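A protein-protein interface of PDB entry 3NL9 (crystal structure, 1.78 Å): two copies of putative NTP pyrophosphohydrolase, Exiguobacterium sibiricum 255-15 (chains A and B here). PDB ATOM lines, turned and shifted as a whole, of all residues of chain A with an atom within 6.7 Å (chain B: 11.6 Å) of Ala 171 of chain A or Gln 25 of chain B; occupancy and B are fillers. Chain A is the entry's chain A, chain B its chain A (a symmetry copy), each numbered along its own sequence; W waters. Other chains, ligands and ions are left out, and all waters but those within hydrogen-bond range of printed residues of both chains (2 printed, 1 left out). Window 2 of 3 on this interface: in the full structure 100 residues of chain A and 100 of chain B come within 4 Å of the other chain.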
ATOM      1  N   GLU A 111     -16.189  14.475 -18.211  1.00  0.00           N
ATOM      2  CA  GLU A 111     -17.353  14.546 -17.317  1.00  0.00           C
ATOM      3  C   GLU A 111     -16.952  14.232 -15.881  1.00  0.00           C
ATOM      4  O   GLU A 111     -17.562  14.731 -14.972  1.00  0.00           O
ATOM      5  CB  GLU A 111     -18.477  13.623 -17.787  1.00  0.00           C
ATOM      6  CG  GLU A 111     -19.043  14.069 -19.100  1.00  0.00           C
ATOM      7  CD  GLU A 111     -20.475  13.689 -19.335  1.00  0.00           C
ATOM      8  OE1 GLU A 111     -21.247  13.433 -18.362  1.00  0.00           O
ATOM      9  OE2 GLU A 111     -20.827  13.699 -20.531  1.00  0.00           O
ATOM     10  N   ALA A 112     -15.914  13.416 -15.711  1.00  0.00           N
ATOM     11  CA  ALA A 112     -15.364  13.081 -14.396  1.00  0.00           C
ATOM     12  C   ALA A 112     -14.439  14.191 -13.883  1.00  0.00           C
ATOM     13  O   ALA A 112     -14.102  14.211 -12.704  1.00  0.00           O
ATOM     14  CB  ALA A 112     -14.580  11.772 -14.483  1.00  0.00           C
ATOM     15  N   GLY A 113     -13.999  15.084 -14.776  1.00  0.00           N
ATOM     16  CA  GLY A 113     -13.006  16.096 -14.428  1.00  0.00           C
ATOM     17  C   GLY A 113     -11.629  15.530 -14.097  1.00  0.00           C
ATOM     18  O   GLY A 113     -10.905  16.087 -13.270  1.00  0.00           O
ATOM     19  N   LEU A 114     -11.291  14.410 -14.721  1.00  0.00           N
ATOM     20  CA  LEU A 114      -9.987  13.780 -14.549  1.00  0.00           C
ATOM     21  C   LEU A 114      -9.154  13.901 -15.814  1.00  0.00           C
ATOM     22  O   LEU A 114      -9.624  13.582 -16.935  1.00  0.00           O
ATOM     23  CB  LEU A 114     -10.113  12.291 -14.204  1.00  0.00           C
ATOM     24  CG  LEU A 114     -10.493  11.838 -12.803  1.00  0.00           C
ATOM     25  CD1 LEU A 114     -10.766  10.324 -12.872  1.00  0.00           C
ATOM     26  CD2 LEU A 114      -9.420  12.187 -11.770  1.00  0.00           C
ATOM     27  N   GLN A 166      -4.887  15.110  -8.176  1.00  0.00           N
ATOM     28  CA  GLN A 166      -5.718  15.973  -9.029  1.00  0.00           C
ATOM     29  C   GLN A 166      -6.834  16.694  -8.266  1.00  0.00           C
ATOM     30  O   GLN A 166      -7.057  17.898  -8.489  1.00  0.00           O
ATOM     31  CB  GLN A 166      -6.317  15.199 -10.188  1.00  0.00           C
ATOM     32  CG  GLN A 166      -5.283  14.726 -11.176  1.00  0.00           C
ATOM     33  CD  GLN A 166      -5.906  14.235 -12.466  1.00  0.00           C
ATOM     34  OE1 GLN A 166      -6.954  14.721 -12.878  1.00  0.00           O
ATOM     35  NE2 GLN A 166      -5.256  13.276 -13.105  1.00  0.00           N
ATOM     36  N   MET A 167      -7.478  15.991  -7.338  1.00  0.00           N
ATOM     37  CA  MET A 167      -8.478  16.621  -6.479  1.00  0.00           C
ATOM     38  C   MET A 167      -7.848  17.772  -5.715  1.00  0.00           C
ATOM     39  O   MET A 167      -8.435  18.868  -5.631  1.00  0.00           O
ATOM     40  CB  MET A 167      -9.084  15.631  -5.472  1.00  0.00           C
ATOM     41  CG  MET A 167      -9.952  14.523  -6.096  1.00  0.00           C
ATOM     42  SD  MET A 167     -10.500  13.154  -4.813  1.00  0.00           S
ATOM     43  CE  MET A 167     -11.599  14.225  -3.590  1.00  0.00           C
ATOM     44  N   LYS A 168      -6.654  17.536  -5.164  1.00  0.00           N
ATOM     45  CA  LYS A 168      -5.934  18.599  -4.428  1.00  0.00           C
ATOM     46  C   LYS A 168      -5.514  19.787  -5.305  1.00  0.00           C
ATOM     47  O   LYS A 168      -5.655  20.946  -4.897  1.00  0.00           O
ATOM     48  CB  LYS A 168      -4.703  18.030  -3.716  1.00  0.00           C
ATOM     49  CG  LYS A 168      -5.026  17.206  -2.493  1.00  0.00           C
ATOM     50  CD  LYS A 168      -3.737  16.830  -1.753  1.00  0.00           C
ATOM     51  CE  LYS A 168      -3.931  15.606  -0.876  1.00  0.00           C
ATOM     52  NZ  LYS A 168      -2.615  15.017  -0.508  1.00  0.00           N
ATOM     53  N   GLU A 169      -4.981  19.493  -6.489  1.00  0.00           N
ATOM     54  CA  GLU A 169      -4.598  20.516  -7.458  1.00  0.00           C
ATOM     55  C   GLU A 169      -5.774  21.413  -7.869  1.00  0.00           C
ATOM     56  O   GLU A 169      -5.607  22.629  -8.032  1.00  0.00           O
ATOM     57  CB  GLU A 169      -3.978  19.834  -8.684  1.00  0.00           C
ATOM     58  CG  GLU A 169      -3.416  20.764  -9.771  1.00  0.00           C
ATOM     59  CD  GLU A 169      -2.992  19.991 -11.025  1.00  0.00           C
ATOM     60  OE1 GLU A 169      -3.864  19.654 -11.862  1.00  0.00           O
ATOM     61  OE2 GLU A 169      -1.786  19.706 -11.169  1.00  0.00           O
ATOM     62  N   LYS A 170      -6.961  20.824  -8.013  1.00  0.00           N
ATOM     63  CA  LYS A 170      -8.143  21.545  -8.506  1.00  0.00           C
ATOM     64  C   LYS A 170      -9.000  22.157  -7.403  1.00  0.00           C
ATOM     65  O   LYS A 170      -9.870  22.991  -7.667  1.00  0.00           O
ATOM     66  CB  LYS A 170      -8.994  20.617  -9.381  1.00  0.00           C
ATOM     67  CG  LYS A 170      -8.289  20.142 -10.660  1.00  0.00           C
ATOM     68  CD  LYS A 170      -7.856  21.299 -11.565  1.00  0.00           C
ATOM     69  CE  LYS A 170      -7.614  20.858 -13.006  1.00  0.00           C
ATOM     70  NZ  LYS A 170      -6.654  19.716 -13.128  1.00  0.00           N
ATOM     71  N   ALA A 171      -8.746  21.759  -6.161  1.00  0.00           N
ATOM     72  CA  ALA A 171      -9.341  22.431  -5.025  1.00  0.00           C
ATOM     73  C   ALA A 171      -8.976  23.927  -5.088  1.00  0.00           C
ATOM     74  O   ALA A 171      -7.839  24.308  -5.424  1.00  0.00           O
ATOM     75  CB  ALA A 171      -8.853  21.801  -3.707  1.00  0.00           C
ATOM     76  OXT ALA A 171      -9.824  24.787  -4.822  1.00  0.00           O
ATOM     77  N   TYR B   8      -7.713  15.184 -24.647  1.00  0.00           N
ATOM     78  CA  TYR B   8      -8.578  15.568 -23.536  1.00  0.00           C
ATOM     79  C   TYR B   8      -9.016  17.034 -23.656  1.00  0.00           C
ATOM     80  O   TYR B   8     -10.190  17.370 -23.424  1.00  0.00           O
ATOM     81  CB  TYR B   8      -7.850  15.305 -22.185  1.00  0.00           C
ATOM     82  CG  TYR B   8      -8.625  15.776 -20.962  1.00  0.00           C
ATOM     83  CD1 TYR B   8      -9.732  15.074 -20.476  1.00  0.00           C
ATOM     84  CD2 TYR B   8      -8.279  16.956 -20.328  1.00  0.00           C
ATOM     85  CE1 TYR B   8     -10.446  15.541 -19.338  1.00  0.00           C
ATOM     86  CE2 TYR B   8      -8.971  17.416 -19.221  1.00  0.00           C
ATOM     87  CZ  TYR B   8     -10.055  16.711 -18.730  1.00  0.00           C
ATOM     88  OH  TYR B   8     -10.719  17.200 -17.617  1.00  0.00           O
ATOM     89  N   LYS B  12     -12.777  18.352 -24.135  1.00  0.00           N
ATOM     90  CA  LYS B  12     -13.220  19.307 -23.134  1.00  0.00           C
ATOM     91  C   LYS B  12     -13.782  20.553 -23.816  1.00  0.00           C
ATOM     92  O   LYS B  12     -14.844  21.090 -23.447  1.00  0.00           O
ATOM     93  CB  LYS B  12     -12.049  19.652 -22.215  1.00  0.00           C
ATOM     94  CG  LYS B  12     -12.432  20.565 -21.070  1.00  0.00           C
ATOM     95  CD  LYS B  12     -11.308  20.676 -20.066  1.00  0.00           C
ATOM     96  CE  LYS B  12     -11.622  21.787 -19.075  1.00  0.00           C
ATOM     97  NZ  LYS B  12     -10.708  21.750 -17.913  1.00  0.00           N
ATOM     98  N   GLN B  16     -17.680  22.158 -23.691  1.00  0.00           N
ATOM     99  CA  GLN B  16     -18.015  23.563 -23.345  1.00  0.00           C
ATOM    100  C   GLN B  16     -18.805  24.157 -24.503  1.00  0.00           C
ATOM    101  O   GLN B  16     -19.878  24.684 -24.300  1.00  0.00           O
ATOM    102  CB  GLN B  16     -16.769  24.444 -23.085  1.00  0.00           C
ATOM    103  CG  GLN B  16     -15.945  24.070 -21.814  1.00  0.00           C
ATOM    104  CD  GLN B  16     -14.683  24.946 -21.594  1.00  0.00           C
ATOM    105  OE1 GLN B  16     -14.780  26.147 -21.323  1.00  0.00           O
ATOM    106  NE2 GLN B  16     -13.501  24.329 -21.708  1.00  0.00           N
ATOM    107  N   PRO B  21     -21.921  18.154 -20.277  1.00  0.00           N
ATOM    108  CA  PRO B  21     -21.384  18.253 -18.929  1.00  0.00           C
ATOM    109  C   PRO B  21     -19.877  18.236 -18.894  1.00  0.00           C
ATOM    110  O   PRO B  21     -19.228  17.541 -19.702  1.00  0.00           O
ATOM    111  CB  PRO B  21     -21.957  17.003 -18.213  1.00  0.00           C
ATOM    112  CG  PRO B  21     -23.205  16.662 -18.979  1.00  0.00           C
ATOM    113  CD  PRO B  21     -22.903  17.043 -20.403  1.00  0.00           C
ATOM    114  N   GLY B  22     -19.330  18.994 -17.956  1.00  0.00           N
ATOM    115  CA  GLY B  22     -17.915  18.966 -17.669  1.00  0.00           C
ATOM    116  C   GLY B  22     -17.678  19.380 -16.224  1.00  0.00           C
ATOM    117  O   GLY B  22     -18.251  20.348 -15.765  1.00  0.00           O
ATOM    118  N   ALA B  23     -16.817  18.665 -15.521  1.00  0.00           N
ATOM    119  CA  ALA B  23     -16.422  19.037 -14.141  1.00  0.00           C
ATOM    120  C   ALA B  23     -15.034  19.710 -14.070  1.00  0.00           C
ATOM    121  O   ALA B  23     -14.062  19.215 -14.631  1.00  0.00           O
ATOM    122  CB  ALA B  23     -16.457  17.811 -13.232  1.00  0.00           C
ATOM    123  N   ASP B  24     -14.968  20.821 -13.346  1.00  0.00           N
ATOM    124  CA  ASP B  24     -13.725  21.575 -13.115  1.00  0.00           C
ATOM    125  C   ASP B  24     -12.881  20.978 -11.999  1.00  0.00           C
ATOM    126  O   ASP B  24     -11.666  21.182 -11.957  1.00  0.00           O
ATOM    127  CB  ASP B  24     -14.049  23.020 -12.731  1.00  0.00           C
ATOM    128  CG  ASP B  24     -14.858  23.743 -13.789  1.00  0.00           C
ATOM    129  OD1 ASP B  24     -14.792  23.349 -14.984  1.00  0.00           O
ATOM    130  OD2 ASP B  24     -15.554  24.713 -13.413  1.00  0.00           O
ATOM    131  N   GLN B  25     -13.556  20.294 -11.078  1.00  0.00           N
ATOM    132  CA  GLN B  25     -12.932  19.491 -10.041  1.00  0.00           C
ATOM    133  C   GLN B  25     -13.272  18.020 -10.300  1.00  0.00           C
ATOM    134  O   GLN B  25     -14.384  17.711 -10.733  1.00  0.00           O
ATOM    135  CB  GLN B  25     -13.449  19.934  -8.682  1.00  0.00           C
ATOM    136  CG  GLN B  25     -13.082  21.370  -8.383  1.00  0.00           C
ATOM    137  CD  GLN B  25     -13.298  21.721  -6.945  1.00  0.00           C
ATOM    138  OE1 GLN B  25     -12.588  21.234  -6.059  1.00  0.00           O
ATOM    139  NE2 GLN B  25     -14.284  22.569  -6.691  1.00  0.00           N
ATOM    140  N   PRO B  26     -12.318  17.113 -10.056  1.00  0.00           N
ATOM    141  CA  PRO B  26     -12.621  15.685 -10.139  1.00  0.00           C
ATOM    142  C   PRO B  26     -13.908  15.337  -9.376  1.00  0.00           C
ATOM    143  O   PRO B  26     -14.041  15.672  -8.202  1.00  0.00           O
ATOM    144  CB  PRO B  26     -11.379  15.036  -9.524  1.00  0.00           C
ATOM    145  CG  PRO B  26     -10.287  16.029  -9.821  1.00  0.00           C
ATOM    146  CD  PRO B  26     -10.928  17.347  -9.620  1.00  0.00           C
ATOM    147  N   THR B  27     -14.854  14.713 -10.073  1.00  0.00           N
ATOM    148  CA  THR B  27     -16.193  14.417  -9.545  1.00  0.00           C
ATOM    149  C   THR B  27     -16.668  13.067 -10.090  1.00  0.00           C
ATOM    150  O   THR B  27     -16.659  12.869 -11.286  1.00  0.00           O
ATOM    151  CB  THR B  27     -17.216  15.477  -9.983  1.00  0.00           C
ATOM    152  OG1 THR B  27     -16.862  16.773  -9.469  1.00  0.00           O
ATOM    153  CG2 THR B  27     -18.609  15.107  -9.480  1.00  0.00           C
ATOM    154  N   ALA B  28     -17.101  12.160  -9.218  1.00  0.00           N
ATOM    155  CA  ALA B  28     -17.655  10.879  -9.670  1.00  0.00           C
ATOM    156  C   ALA B  28     -18.830  11.120 -10.623  1.00  0.00           C
ATOM    157  O   ALA B  28     -19.680  11.935 -10.335  1.00  0.00           O
ATOM    158  CB  ALA B  28     -18.134  10.014  -8.472  1.00  0.00           C
ATOM    159  N   ILE B  29     -18.888  10.373 -11.714  1.00  0.00           N
ATOM    160  CA  ILE B  29     -19.993  10.490 -12.682  1.00  0.00           C
ATOM    161  C   ILE B  29     -21.235   9.774 -12.091  1.00  0.00           C
ATOM    162  O   ILE B  29     -21.159   8.591 -11.723  1.00  0.00           O
ATOM    163  CB  ILE B  29     -19.600   9.881 -14.057  1.00  0.00           C
ATOM    164  CG1 ILE B  29     -18.419  10.622 -14.674  1.00  0.00           C
ATOM    165  CG2 ILE B  29     -20.787   9.936 -15.040  1.00  0.00           C
ATOM    166  CD1 ILE B  29     -17.798   9.885 -15.848  1.00  0.00           C
ATOM    167  N   PRO B  30     -22.381  10.486 -11.958  1.00  0.00           N
ATOM    168  CA  PRO B  30     -23.609   9.784 -11.507  1.00  0.00           C
ATOM    169  C   PRO B  30     -23.984   8.568 -12.349  1.00  0.00           C
ATOM    170  O   PRO B  30     -23.796   8.593 -13.560  1.00  0.00           O
ATOM    171  CB  PRO B  30     -24.696  10.858 -11.641  1.00  0.00           C
ATOM    172  CG  PRO B  30     -23.940  12.166 -11.596  1.00  0.00           C
ATOM    173  CD  PRO B  30     -22.666  11.885 -12.317  1.00  0.00           C
ATOM    174  N   GLU B  87     -18.028   8.482  -2.431  1.00  0.00           N
ATOM    175  CA  GLU B  87     -17.971   9.140  -3.734  1.00  0.00           C
ATOM    176  C   GLU B  87     -16.536   9.140  -4.290  1.00  0.00           C
ATOM    177  O   GLU B  87     -16.308   8.914  -5.473  1.00  0.00           O
ATOM    178  CB  GLU B  87     -18.520  10.553  -3.593  1.00  0.00           C
ATOM    179  CG  GLU B  87     -18.910  11.213  -4.891  1.00  0.00           C
ATOM    180  CD  GLU B  87     -19.524  12.600  -4.673  1.00  0.00           C
ATOM    181  OE1 GLU B  87     -20.254  12.774  -3.662  1.00  0.00           O
ATOM    182  OE2 GLU B  87     -19.270  13.506  -5.512  1.00  0.00           O
ATOM    183  N   VAL B  88     -15.552   9.309  -3.411  1.00  0.00           N
ATOM    184  CA  VAL B  88     -14.180   9.235  -3.857  1.00  0.00           C
ATOM    185  C   VAL B  88     -13.883   7.853  -4.405  1.00  0.00           C
ATOM    186  O   VAL B  88     -13.283   7.757  -5.456  1.00  0.00           O
ATOM    187  CB  VAL B  88     -13.176   9.588  -2.755  1.00  0.00           C
ATOM    188  CG1 VAL B  88     -11.766   9.224  -3.229  1.00  0.00           C
ATOM    189  CG2 VAL B  88     -13.281  11.068  -2.446  1.00  0.00           C
ATOM    190  N   LEU B  91     -15.225   7.588  -7.889  1.00  0.00           N
ATOM    191  CA  LEU B  91     -14.391   8.345  -8.858  1.00  0.00           C
ATOM    192  C   LEU B  91     -13.120   7.578  -9.209  1.00  0.00           C
ATOM    193  O   LEU B  91     -12.718   7.468 -10.376  1.00  0.00           O
ATOM    194  CB  LEU B  91     -14.029   9.731  -8.278  1.00  0.00           C
ATOM    195  CG  LEU B  91     -13.145  10.680  -9.095  1.00  0.00           C
ATOM    196  CD1 LEU B  91     -13.826  11.058 -10.442  1.00  0.00           C
ATOM    197  CD2 LEU B  91     -12.786  11.914  -8.259  1.00  0.00           C
ATOM    198  N   VAL B  92     -12.496   7.026  -8.177  1.00  0.00           N
ATOM    199  CA  VAL B  92     -11.253   6.302  -8.368  1.00  0.00           C
ATOM    200  C   VAL B  92     -11.490   5.089  -9.257  1.00  0.00           C
ATOM    201  O   VAL B  92     -10.740   4.861 -10.206  1.00  0.00           O
ATOM    202  CB  VAL B  92     -10.651   5.908  -7.018  1.00  0.00           C
ATOM    203  CG1 VAL B  92      -9.494   4.957  -7.182  1.00  0.00           C
ATOM    204  CG2 VAL B  92     -10.263   7.156  -6.263  1.00  0.00           C
ATOM    205  N   GLN B  94     -13.947   4.554 -11.440  1.00  0.00           N
ATOM    206  CA  GLN B  94     -14.264   5.030 -12.781  1.00  0.00           C
ATOM    207  C   GLN B  94     -12.996   5.403 -13.554  1.00  0.00           C
ATOM    208  O   GLN B  94     -12.802   4.977 -14.706  1.00  0.00           O
ATOM    209  CB  GLN B  94     -15.184   6.245 -12.688  1.00  0.00           C
ATOM    210  CG  GLN B  94     -16.592   5.890 -12.370  1.00  0.00           C
ATOM    211  CD  GLN B  94     -17.465   7.076 -11.990  1.00  0.00           C
ATOM    212  OE1 GLN B  94     -16.987   8.182 -11.869  1.00  0.00           O
ATOM    213  NE2 GLN B  94     -18.764   6.839 -11.812  1.00  0.00           N
HETATM  214  O   HOH W   1     -11.011  19.072  -6.175  1.00  0.00           O
HETATM  215  O   HOH W   2     -10.567  18.920 -13.926  1.00  0.00           O
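No position is printed for both chains. Of the 17 pairs that touch across the chains among the printed residues, none has its exchanged pair printed and touching as well.
The side-chain carboxylate (OE1) of Glu 169 of chain A lies within salt-bridge range of the side-chain amino group (NZ) of Lys 170 of chain A, 3.1 Å away. OG1 of Thr 27 of chain B sits at hydrogen-bond distance from O of Gln 25 of chain B. The backbone NH (N) of Ile 29 of chain B is in hydrogen-bond range of the side-chain amide oxygen (OE1) of Gln 94 of chain B, at 2.9 Å.
N of Thr 27 of chain B lies within hydrogen-bond range of O of Ala 112 of chain A (2.8 Å).
Among the printed residues, pairs that only touch across the chains: Leu 114 of chain A with Tyr 8 of chain B (3.2 Å), Gly 113 of chain A with Ala 23 of chain B (3.3 Å), Ala 112 of chain A with Pro 26 of chain B (3.3 Å), Gly 113 of chain A with Pro 26 of chain B (3.5 Å), Glu 111 of chain A with Pro 21 of chain B (3.5 Å), Ala 171 of chain A with Gln 25 of chain B (3.6 Å), Lys 170 of chain A with Gln 25 of chain B (3.6 Å), Glu 111 of chain A with Ala 23 of chain B (3.7 Å), Met 167 of chain A with Pro 26 of chain B (3.7 Å), Lys 170 of chain A with Asp 24 of chain B (3.8 Å), Met 167 of chain A with Val 88 of chain B (3.8 Å), Lys 170 of chain A with Pro 26 of chain B (3.8 Å), Gln 166 of chain A with Pro 26 of chain B (3.8 Å), Ala 112 of chain A with Leu 91 of chain B (3.9 Å), Ala 112 of chain A with Ile 29 of chain B (3.9 Å) and Leu 114 of chain A with Leu 91 of chain B (3.98 Å).
Of chain B, only Gln 25 (3.6 Å) comes within 4 Å of Ala 171 of chain A. Of chain A, only Lys 170 (3.6 Å) and Ala 171 (3.6 Å) come within 4 Å of Gln 25 of chain B. Of chain B, only Pro 26, Thr 27, Ile 29 and Leu 91 come within 4 Å of Ala 112 of chain A. Printed residues of chain A within 4 Å of Asp 24 of chain B: Lys 170 (3.8 Å). Printed residues of chain B within 4 Å of Leu 114 of chain A: Tyr 8 (3.2 Å) and Leu 91 (3.98 Å). Of the printed residues of chain A, Ile 29 of chain B touches Ala 112 (3.9 Å). Of the printed residues of chain A, Pro 26 of chain B touches Ala 112 (3.3 Å), Gly 113 (3.5 Å), Gln 166 (3.8 Å), Met 167 (3.7 Å) and Lys 170 (3.8 Å). Printed residues of chain B within 4 Å of Gly 113 of chain A: Ala 23 and Pro 26. Pro 30 of chain B touches none of the printed residues of chain A. The nearest residue of chain B that does not touch Ala 171 of chain A is Pro 26 of chain B (6.0 Å).
Among the printed residues, 17 pairs touch across the chains. Among the printed residues, no Asp or Glu carboxylate lies within 4 Å of a Lys or Arg side-chain nitrogen of the other chain.
Water W1 lies within hydrogen-bond range of O of Met 167 of chain A (2.6 Å) and OE1 of Gln 25 of chain B (2.7 Å). Water W2 bridges O of Gly 113 of chain A (2.9 Å) and O of Asp 24 of chain B (3.2 Å).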
